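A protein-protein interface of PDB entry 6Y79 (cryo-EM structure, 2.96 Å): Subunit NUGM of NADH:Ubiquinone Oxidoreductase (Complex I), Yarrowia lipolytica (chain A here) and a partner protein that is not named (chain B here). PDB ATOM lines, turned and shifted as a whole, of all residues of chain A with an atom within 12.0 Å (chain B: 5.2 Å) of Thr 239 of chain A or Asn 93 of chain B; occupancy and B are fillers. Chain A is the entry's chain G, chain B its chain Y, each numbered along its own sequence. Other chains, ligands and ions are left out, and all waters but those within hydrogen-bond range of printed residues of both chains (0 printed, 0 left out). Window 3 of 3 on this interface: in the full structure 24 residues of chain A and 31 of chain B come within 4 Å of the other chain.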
ATOM      1  N   THR A 217     -10.967 -25.320  -2.056  1.00  0.00           N
ATOM      2  CA  THR A 217     -11.259 -23.994  -1.552  1.00  0.00           C
ATOM      3  C   THR A 217      -9.986 -23.161  -1.420  1.00  0.00           C
ATOM      4  O   THR A 217     -10.060 -21.936  -1.313  1.00  0.00           O
ATOM      5  CB  THR A 217     -12.018 -24.178  -0.240  1.00  0.00           C
ATOM      6  OG1 THR A 217     -13.017 -25.177  -0.444  1.00  0.00           O
ATOM      7  CG2 THR A 217     -12.741 -22.960   0.166  1.00  0.00           C
ATOM      8  N   THR A 220      -6.036 -19.457   1.182  1.00  0.00           N
ATOM      9  CA  THR A 220      -6.289 -18.153   1.770  1.00  0.00           C
ATOM     10  C   THR A 220      -7.715 -17.701   1.493  1.00  0.00           C
ATOM     11  O   THR A 220      -8.431 -18.264   0.666  1.00  0.00           O
ATOM     12  CB  THR A 220      -5.317 -17.097   1.232  1.00  0.00           C
ATOM     13  OG1 THR A 220      -5.552 -16.898  -0.165  1.00  0.00           O
ATOM     14  CG2 THR A 220      -3.879 -17.517   1.440  1.00  0.00           C
ATOM     15  N   GLU A 221      -8.103 -16.650   2.208  1.00  0.00           N
ATOM     16  CA  GLU A 221      -9.383 -15.982   2.050  1.00  0.00           C
ATOM     17  C   GLU A 221      -9.174 -14.493   2.277  1.00  0.00           C
ATOM     18  O   GLU A 221      -8.113 -14.057   2.716  1.00  0.00           O
ATOM     19  CB  GLU A 221     -10.431 -16.541   3.013  1.00  0.00           C
ATOM     20  CG  GLU A 221     -10.079 -16.347   4.463  1.00  0.00           C
ATOM     21  CD  GLU A 221     -11.109 -16.935   5.390  1.00  0.00           C
ATOM     22  OE1 GLU A 221     -12.083 -17.528   4.884  1.00  0.00           O
ATOM     23  OE2 GLU A 221     -10.952 -16.801   6.626  1.00  0.00           O
ATOM     24  N   VAL A 222     -10.205 -13.710   1.982  1.00  0.00           N
ATOM     25  CA  VAL A 222     -10.129 -12.253   1.945  1.00  0.00           C
ATOM     26  C   VAL A 222     -11.194 -11.690   2.872  1.00  0.00           C
ATOM     27  O   VAL A 222     -12.330 -12.174   2.876  1.00  0.00           O
ATOM     28  CB  VAL A 222     -10.336 -11.731   0.508  1.00  0.00           C
ATOM     29  CG1 VAL A 222     -10.368 -10.224   0.449  1.00  0.00           C
ATOM     30  CG2 VAL A 222      -9.257 -12.244  -0.390  1.00  0.00           C
ATOM     31  N   ARG A 223     -10.834 -10.682   3.668  1.00  0.00           N
ATOM     32  CA  ARG A 223     -11.869  -9.889   4.323  1.00  0.00           C
ATOM     33  C   ARG A 223     -11.410  -8.444   4.399  1.00  0.00           C
ATOM     34  O   ARG A 223     -10.276  -8.124   4.068  1.00  0.00           O
ATOM     35  CB  ARG A 223     -12.218 -10.431   5.709  1.00  0.00           C
ATOM     36  CG  ARG A 223     -11.131 -10.306   6.724  1.00  0.00           C
ATOM     37  CD  ARG A 223     -11.636 -10.745   8.073  1.00  0.00           C
ATOM     38  NE  ARG A 223     -10.570 -10.739   9.062  1.00  0.00           N
ATOM     39  CZ  ARG A 223     -10.275  -9.702   9.832  1.00  0.00           C
ATOM     40  NH1 ARG A 223      -9.278  -9.792  10.694  1.00  0.00           N
ATOM     41  NH2 ARG A 223     -10.967  -8.579   9.736  1.00  0.00           N
ATOM     42  N   GLU A 234      -5.995 -13.909   4.678  1.00  0.00           N
ATOM     43  CA  GLU A 234      -5.830 -14.719   5.871  1.00  0.00           C
ATOM     44  C   GLU A 234      -5.813 -16.186   5.488  1.00  0.00           C
ATOM     45  O   GLU A 234      -6.225 -16.541   4.382  1.00  0.00           O
ATOM     46  CB  GLU A 234      -6.973 -14.441   6.853  1.00  0.00           C
ATOM     47  CG  GLU A 234      -6.784 -13.163   7.614  1.00  0.00           C
ATOM     48  CD  GLU A 234      -7.869 -12.939   8.627  1.00  0.00           C
ATOM     49  OE1 GLU A 234      -8.452 -11.842   8.618  1.00  0.00           O
ATOM     50  OE2 GLU A 234      -8.141 -13.853   9.430  1.00  0.00           O
ATOM     51  N   PRO A 235      -5.308 -17.060   6.357  1.00  0.00           N
ATOM     52  CA  PRO A 235      -5.501 -18.494   6.132  1.00  0.00           C
ATOM     53  C   PRO A 235      -6.970 -18.863   6.209  1.00  0.00           C
ATOM     54  O   PRO A 235      -7.771 -18.239   6.906  1.00  0.00           O
ATOM     55  CB  PRO A 235      -4.696 -19.153   7.255  1.00  0.00           C
ATOM     56  CG  PRO A 235      -4.421 -18.084   8.215  1.00  0.00           C
ATOM     57  CD  PRO A 235      -4.330 -16.830   7.428  1.00  0.00           C
ATOM     58  N   LEU A 236      -7.313 -19.900   5.462  1.00  0.00           N
ATOM     59  CA  LEU A 236      -8.697 -20.152   5.110  1.00  0.00           C
ATOM     60  C   LEU A 236      -9.451 -20.830   6.239  1.00  0.00           C
ATOM     61  O   LEU A 236      -8.903 -21.654   6.974  1.00  0.00           O
ATOM     62  CB  LEU A 236      -8.750 -21.010   3.859  1.00  0.00           C
ATOM     63  CG  LEU A 236     -10.073 -21.461   3.268  1.00  0.00           C
ATOM     64  CD1 LEU A 236     -10.934 -20.295   2.865  1.00  0.00           C
ATOM     65  CD2 LEU A 236      -9.706 -22.262   2.090  1.00  0.00           C
ATOM     66  N   GLU A 237     -10.724 -20.471   6.361  1.00  0.00           N
ATOM     67  CA  GLU A 237     -11.602 -21.045   7.362  1.00  0.00           C
ATOM     68  C   GLU A 237     -13.028 -20.901   6.864  1.00  0.00           C
ATOM     69  O   GLU A 237     -13.403 -19.831   6.380  1.00  0.00           O
ATOM     70  CB  GLU A 237     -11.406 -20.333   8.684  1.00  0.00           C
ATOM     71  CG  GLU A 237     -11.937 -21.068   9.839  1.00  0.00           C
ATOM     72  CD  GLU A 237     -11.823 -20.258  11.076  1.00  0.00           C
ATOM     73  OE1 GLU A 237     -11.264 -19.146  11.019  1.00  0.00           O
ATOM     74  OE2 GLU A 237     -12.312 -20.729  12.104  1.00  0.00           O
ATOM     75  N   LEU A 238     -13.812 -21.969   6.976  1.00  0.00           N
ATOM     76  CA  LEU A 238     -15.139 -22.035   6.391  1.00  0.00           C
ATOM     77  C   LEU A 238     -16.199 -22.184   7.470  1.00  0.00           C
ATOM     78  O   LEU A 238     -15.977 -22.835   8.492  1.00  0.00           O
ATOM     79  CB  LEU A 238     -15.238 -23.204   5.412  1.00  0.00           C
ATOM     80  CG  LEU A 238     -14.381 -23.091   4.151  1.00  0.00           C
ATOM     81  CD1 LEU A 238     -14.439 -24.361   3.348  1.00  0.00           C
ATOM     82  CD2 LEU A 238     -14.823 -21.925   3.311  1.00  0.00           C
ATOM     83  N   THR A 239     -17.358 -21.575   7.231  1.00  0.00           N
ATOM     84  CA  THR A 239     -18.472 -21.732   8.151  1.00  0.00           C
ATOM     85  C   THR A 239     -19.191 -23.050   7.900  1.00  0.00           C
ATOM     86  O   THR A 239     -19.686 -23.672   8.839  1.00  0.00           O
ATOM     87  CB  THR A 239     -19.398 -20.514   8.036  1.00  0.00           C
ATOM     88  OG1 THR A 239     -18.643 -19.331   8.311  1.00  0.00           O
ATOM     89  CG2 THR A 239     -20.537 -20.572   9.021  1.00  0.00           C
ATOM     90  N   GLN A 240     -19.198 -23.528   6.662  1.00  0.00           N
ATOM     91  CA  GLN A 240     -19.583 -24.899   6.373  1.00  0.00           C
ATOM     92  C   GLN A 240     -18.454 -25.568   5.616  1.00  0.00           C
ATOM     93  O   GLN A 240     -18.011 -25.056   4.586  1.00  0.00           O
ATOM     94  CB  GLN A 240     -20.863 -24.975   5.563  1.00  0.00           C
ATOM     95  CG  GLN A 240     -21.451 -26.351   5.584  1.00  0.00           C
ATOM     96  CD  GLN A 240     -22.773 -26.409   4.913  1.00  0.00           C
ATOM     97  OE1 GLN A 240     -23.204 -25.447   4.293  1.00  0.00           O
ATOM     98  NE2 GLN A 240     -23.449 -27.535   5.042  1.00  0.00           N
ATOM     99  N   ALA A 241     -17.986 -26.698   6.132  1.00  0.00           N
ATOM    100  CA  ALA A 241     -16.900 -27.416   5.490  1.00  0.00           C
ATOM    101  C   ALA A 241     -17.390 -28.077   4.214  1.00  0.00           C
ATOM    102  O   ALA A 241     -18.563 -28.427   4.083  1.00  0.00           O
ATOM    103  CB  ALA A 241     -16.319 -28.466   6.428  1.00  0.00           C
ATOM    104  N   PHE A 242     -16.477 -28.228   3.262  1.00  0.00           N
ATOM    105  CA  PHE A 242     -16.813 -28.865   2.000  1.00  0.00           C
ATOM    106  C   PHE A 242     -17.037 -30.350   2.215  1.00  0.00           C
ATOM    107  O   PHE A 242     -16.242 -31.019   2.876  1.00  0.00           O
ATOM    108  CB  PHE A 242     -15.708 -28.637   0.979  1.00  0.00           C
ATOM    109  CG  PHE A 242     -15.969 -29.277  -0.341  1.00  0.00           C
ATOM    110  CD1 PHE A 242     -16.952 -28.794  -1.175  1.00  0.00           C
ATOM    111  CD2 PHE A 242     -15.231 -30.362  -0.752  1.00  0.00           C
ATOM    112  CE1 PHE A 242     -17.189 -29.381  -2.391  1.00  0.00           C
ATOM    113  CE2 PHE A 242     -15.469 -30.953  -1.965  1.00  0.00           C
ATOM    114  CZ  PHE A 242     -16.456 -30.461  -2.780  1.00  0.00           C
ATOM    115  N   ARG A 243     -18.136 -30.858   1.678  1.00  0.00           N
ATOM    116  CA  ARG A 243     -18.497 -32.262   1.793  1.00  0.00           C
ATOM    117  C   ARG A 243     -18.461 -32.868   0.406  1.00  0.00           C
ATOM    118  O   ARG A 243     -19.364 -32.623  -0.394  1.00  0.00           O
ATOM    119  CB  ARG A 243     -19.880 -32.424   2.406  1.00  0.00           C
ATOM    120  CG  ARG A 243     -19.934 -32.118   3.869  1.00  0.00           C
ATOM    121  CD  ARG A 243     -21.341 -32.176   4.370  1.00  0.00           C
ATOM    122  NE  ARG A 243     -22.195 -31.251   3.644  1.00  0.00           N
ATOM    123  CZ  ARG A 243     -23.510 -31.194   3.787  1.00  0.00           C
ATOM    124  NH1 ARG A 243     -24.117 -32.014   4.634  1.00  0.00           N
ATOM    125  NH2 ARG A 243     -24.214 -30.324   3.082  1.00  0.00           N
ATOM    126  N   TRP B  91     -15.844 -28.407  13.837  1.00  0.00           N
ATOM    127  CA  TRP B  91     -16.641 -28.006  14.988  1.00  0.00           C
ATOM    128  C   TRP B  91     -18.006 -27.538  14.516  1.00  0.00           C
ATOM    129  O   TRP B  91     -18.162 -27.081  13.384  1.00  0.00           O
ATOM    130  CB  TRP B  91     -15.967 -26.903  15.810  1.00  0.00           C
ATOM    131  CG  TRP B  91     -15.721 -25.620  15.085  1.00  0.00           C
ATOM    132  CD1 TRP B  91     -16.507 -24.515  15.092  1.00  0.00           C
ATOM    133  CD2 TRP B  91     -14.591 -25.303  14.275  1.00  0.00           C
ATOM    134  NE1 TRP B  91     -15.946 -23.532  14.326  1.00  0.00           N
ATOM    135  CE2 TRP B  91     -14.767 -23.994  13.809  1.00  0.00           C
ATOM    136  CE3 TRP B  91     -13.455 -26.009  13.884  1.00  0.00           C
ATOM    137  CZ2 TRP B  91     -13.849 -23.375  12.982  1.00  0.00           C
ATOM    138  CZ3 TRP B  91     -12.547 -25.390  13.065  1.00  0.00           C
ATOM    139  CH2 TRP B  91     -12.745 -24.085  12.626  1.00  0.00           C
ATOM    140  N   GLU B  92     -18.996 -27.651  15.399  1.00  0.00           N
ATOM    141  CA  GLU B  92     -20.362 -27.288  15.052  1.00  0.00           C
ATOM    142  C   GLU B  92     -20.602 -25.802  15.266  1.00  0.00           C
ATOM    143  O   GLU B  92     -20.064 -25.198  16.195  1.00  0.00           O
ATOM    144  CB  GLU B  92     -21.361 -28.097  15.867  1.00  0.00           C
ATOM    145  CG  GLU B  92     -20.953 -28.330  17.298  1.00  0.00           C
ATOM    146  CD  GLU B  92     -21.799 -29.396  17.947  1.00  0.00           C
ATOM    147  OE1 GLU B  92     -22.816 -29.775  17.339  1.00  0.00           O
ATOM    148  OE2 GLU B  92     -21.449 -29.852  19.055  1.00  0.00           O
ATOM    149  N   ASN B  93     -21.431 -25.225  14.410  1.00  0.00           N
ATOM    150  CA  ASN B  93     -21.611 -23.784  14.370  1.00  0.00           C
ATOM    151  C   ASN B  93     -22.501 -23.315  15.514  1.00  0.00           C
ATOM    152  O   ASN B  93     -23.354 -24.066  15.999  1.00  0.00           O
ATOM    153  CB  ASN B  93     -22.217 -23.385  13.022  1.00  0.00           C
ATOM    154  CG  ASN B  93     -22.189 -21.891  12.770  1.00  0.00           C
ATOM    155  OD1 ASN B  93     -21.664 -21.112  13.563  1.00  0.00           O
ATOM    156  ND2 ASN B  93     -22.766 -21.484  11.652  1.00  0.00           N
ATOM    157  N   ASP B  94     -22.256 -22.063  15.949  1.00  0.00           N
ATOM    158  CA  ASP B  94     -23.176 -21.302  16.794  1.00  0.00           C
ATOM    159  C   ASP B  94     -24.607 -21.423  16.325  1.00  0.00           C
ATOM    160  O   ASP B  94     -25.522 -21.697  17.105  1.00  0.00           O
ATOM    161  CB  ASP B  94     -22.879 -19.812  16.693  1.00  0.00           C
ATOM    162  CG  ASP B  94     -21.898 -19.317  17.703  1.00  0.00           C
ATOM    163  OD1 ASP B  94     -21.573 -20.034  18.670  1.00  0.00           O
ATOM    164  OD2 ASP B  94     -21.469 -18.181  17.493  1.00  0.00           O
ATOM    165  N   LEU B  95     -24.795 -21.186  15.048  1.00  0.00           N
ATOM    166  CA  LEU B  95     -26.006 -20.647  14.478  1.00  0.00           C
ATOM    167  C   LEU B  95     -27.021 -21.707  14.104  1.00  0.00           C
ATOM    168  O   LEU B  95     -28.123 -21.760  14.657  1.00  0.00           O
ATOM    169  CB  LEU B  95     -25.595 -19.865  13.251  1.00  0.00           C
ATOM    170  CG  LEU B  95     -26.710 -19.142  12.574  1.00  0.00           C
ATOM    171  CD1 LEU B  95     -27.105 -18.029  13.444  1.00  0.00           C
ATOM    172  CD2 LEU B  95     -26.109 -18.636  11.349  1.00  0.00           C
ATOM    173  N   ILE B  96     -26.637 -22.548  13.145  1.00  0.00           N
ATOM    174  CA  ILE B  96     -27.473 -23.624  12.650  1.00  0.00           C
ATOM    175  C   ILE B  96     -26.869 -24.985  12.960  1.00  0.00           C
ATOM    176  O   ILE B  96     -27.585 -25.981  13.044  1.00  0.00           O
ATOM    177  CB  ILE B  96     -27.722 -23.473  11.137  1.00  0.00           C
ATOM    178  CG1 ILE B  96     -28.058 -22.037  10.795  1.00  0.00           C
ATOM    179  CG2 ILE B  96     -28.931 -24.250  10.713  1.00  0.00           C
ATOM    180  CD1 ILE B  96     -28.182 -21.787   9.334  1.00  0.00           C
ATOM    181  N   GLY B  97     -25.564 -25.054  13.163  1.00  0.00           N
ATOM    182  CA  GLY B  97     -24.984 -26.337  13.481  1.00  0.00           C
ATOM    183  C   GLY B  97     -24.336 -26.933  12.260  1.00  0.00           C
ATOM    184  O   GLY B  97     -24.262 -28.155  12.102  1.00  0.00           O
ATOM    185  N   TRP B  98     -23.903 -26.055  11.370  1.00  0.00           N
ATOM    186  CA  TRP B  98     -23.077 -26.467  10.254  1.00  0.00           C
ATOM    187  C   TRP B  98     -21.736 -26.959  10.760  1.00  0.00           C
ATOM    188  O   TRP B  98     -21.177 -26.422  11.715  1.00  0.00           O
ATOM    189  CB  TRP B  98     -22.857 -25.307   9.301  1.00  0.00           C
ATOM    190  CG  TRP B  98     -24.037 -24.940   8.513  1.00  0.00           C
ATOM    191  CD1 TRP B  98     -25.197 -25.634   8.393  1.00  0.00           C
ATOM    192  CD2 TRP B  98     -24.180 -23.773   7.717  1.00  0.00           C
ATOM    193  NE1 TRP B  98     -26.059 -24.966   7.568  1.00  0.00           N
ATOM    194  CE2 TRP B  98     -25.452 -23.817   7.138  1.00  0.00           C
ATOM    195  CE3 TRP B  98     -23.351 -22.687   7.439  1.00  0.00           C
ATOM    196  CZ2 TRP B  98     -25.916 -22.822   6.298  1.00  0.00           C
ATOM    197  CZ3 TRP B  98     -23.808 -21.706   6.611  1.00  0.00           C
ATOM    198  CH2 TRP B  98     -25.077 -21.775   6.047  1.00  0.00           C
ATOM    199  N   GLN B  99     -21.229 -27.994  10.120  1.00  0.00           N
ATOM    200  CA  GLN B  99     -19.891 -28.485  10.400  1.00  0.00           C
ATOM    201  C   GLN B  99     -18.893 -27.520   9.781  1.00  0.00           C
ATOM    202  O   GLN B  99     -18.696 -27.511   8.568  1.00  0.00           O
ATOM    203  CB  GLN B  99     -19.747 -29.887   9.836  1.00  0.00           C
ATOM    204  CG  GLN B  99     -20.778 -30.829  10.380  1.00  0.00           C
ATOM    205  CD  GLN B  99     -20.491 -31.149  11.801  1.00  0.00           C
ATOM    206  OE1 GLN B  99     -19.336 -31.292  12.174  1.00  0.00           O
ATOM    207  NE2 GLN B  99     -21.526 -31.267  12.610  1.00  0.00           N
ATOM    208  N   SER B 100     -18.274 -26.690  10.614  1.00  0.00           N
ATOM    209  CA  SER B 100     -17.274 -25.721  10.193  1.00  0.00           C
ATOM    210  C   SER B 100     -15.887 -26.319  10.353  1.00  0.00           C
ATOM    211  O   SER B 100     -15.663 -27.163  11.214  1.00  0.00           O
ATOM    212  CB  SER B 100     -17.362 -24.448  11.025  1.00  0.00           C
ATOM    213  OG  SER B 100     -18.633 -23.856  10.907  1.00  0.00           O
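Of the printed residues of chain B, Leu 238 of chain A touches Ser 100 (3.3 Å).
Printed residues of chain B within 4 Å of Thr 239 of chain A: Asn 93 (3.6 Å), Trp 98 (3.6 Å), Gln 99 (3.97 Å) and Ser 100 (2.3 Å).
Of the printed residues of chain B, Gln 240 of chain A touches Trp 98 (3.9 Å) and Gln 99 (3.5 Å).
Of the printed residues of chain B, Ala 241 of chain A touches Gln 99 (2.7 Å).
No residue of chain A comes within 4 Å of Glu 92 of chain B.
No residue of chain A comes within 4 Å of Asp 94 of chain B.
No residue of chain A comes within 4 Å of Ile 96 of chain B.
Gly 97 of chain B touches none of the printed residues of chain A.
Of the printed residues of chain A, Trp 98 of chain B touches Thr 239 and Gln 240.
Gln 99 of chain B touches three residues of chain A.
Ser 100 of chain B touches just these residues of chain A: Leu 238 (3.3 Å) and Thr 239 (2.3 Å).
The nearest printed residue of chain B that does not touch Thr 239 of chain A is Trp 91 of chain B (5.9 Å).
The nearest residue of chain A that does not touch Asn 93 of chain B is Gln 240 of chain A (6.5 Å).
The nearest printed residue of chain B that does not touch Glu 237 of chain A is Ser 100 of chain B (6.4 Å).
Glu 237 of chain A touches Trp 91 of chain B.
CB of Ser 100 of chain B touches O of Leu 238 of chain A, 3.3 Å away.
CG2 of Thr 239 of chain A touches ND2 of Asn 93 of chain B (3.6 Å).
O of Thr 239 of chain A touches CB of Trp 98 of chain B (3.6 Å).
Thr 239 of chain A touches Gln 99 of chain B (O to O, 3.97 Å).
Gln 240 of chain A touches Trp 98 of chain B (CB to CE3, 3.9 Å).
CA of Gln 240 of chain A touches O of Gln 99 of chain B (3.5 Å).
Along chain A the printed residues that touch a printed residue of chain B span positions 237 to 241.
Along chain B the printed residues that touch a printed residue of chain A span positions 91 to 100.
O of Trp 91 of chain B lies within hydrogen-bond range of N of Ser 100 of chain B, 2.8 Å away.
The side-chain amide oxygen (OD1) of Asn 93 of chain B lies close to the backbone NH (N) of Leu 95 of chain B (3.5 Å).
The backbone NH (N) of Asn 93 of chain B sits at hydrogen-bond distance from the backbone carbonyl oxygen (O) of Trp 98 of chain B, at 3.0 Å.
The guanidinium group (NH2) of Arg 243 of chain A lies close to the side-chain amide nitrogen (NE2) of Gln 240 of chain A (3.5 Å).
The backbone NH (N) of Ala 241 of chain A lies within hydrogen-bond range of the backbone carbonyl oxygen (O) of Gln 99 of chain B (2.7 Å).
The backbone carbonyl oxygen (O) of Thr 239 of chain A sits close to the side-chain hydroxyl (OG) of Ser 100 of chain B.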
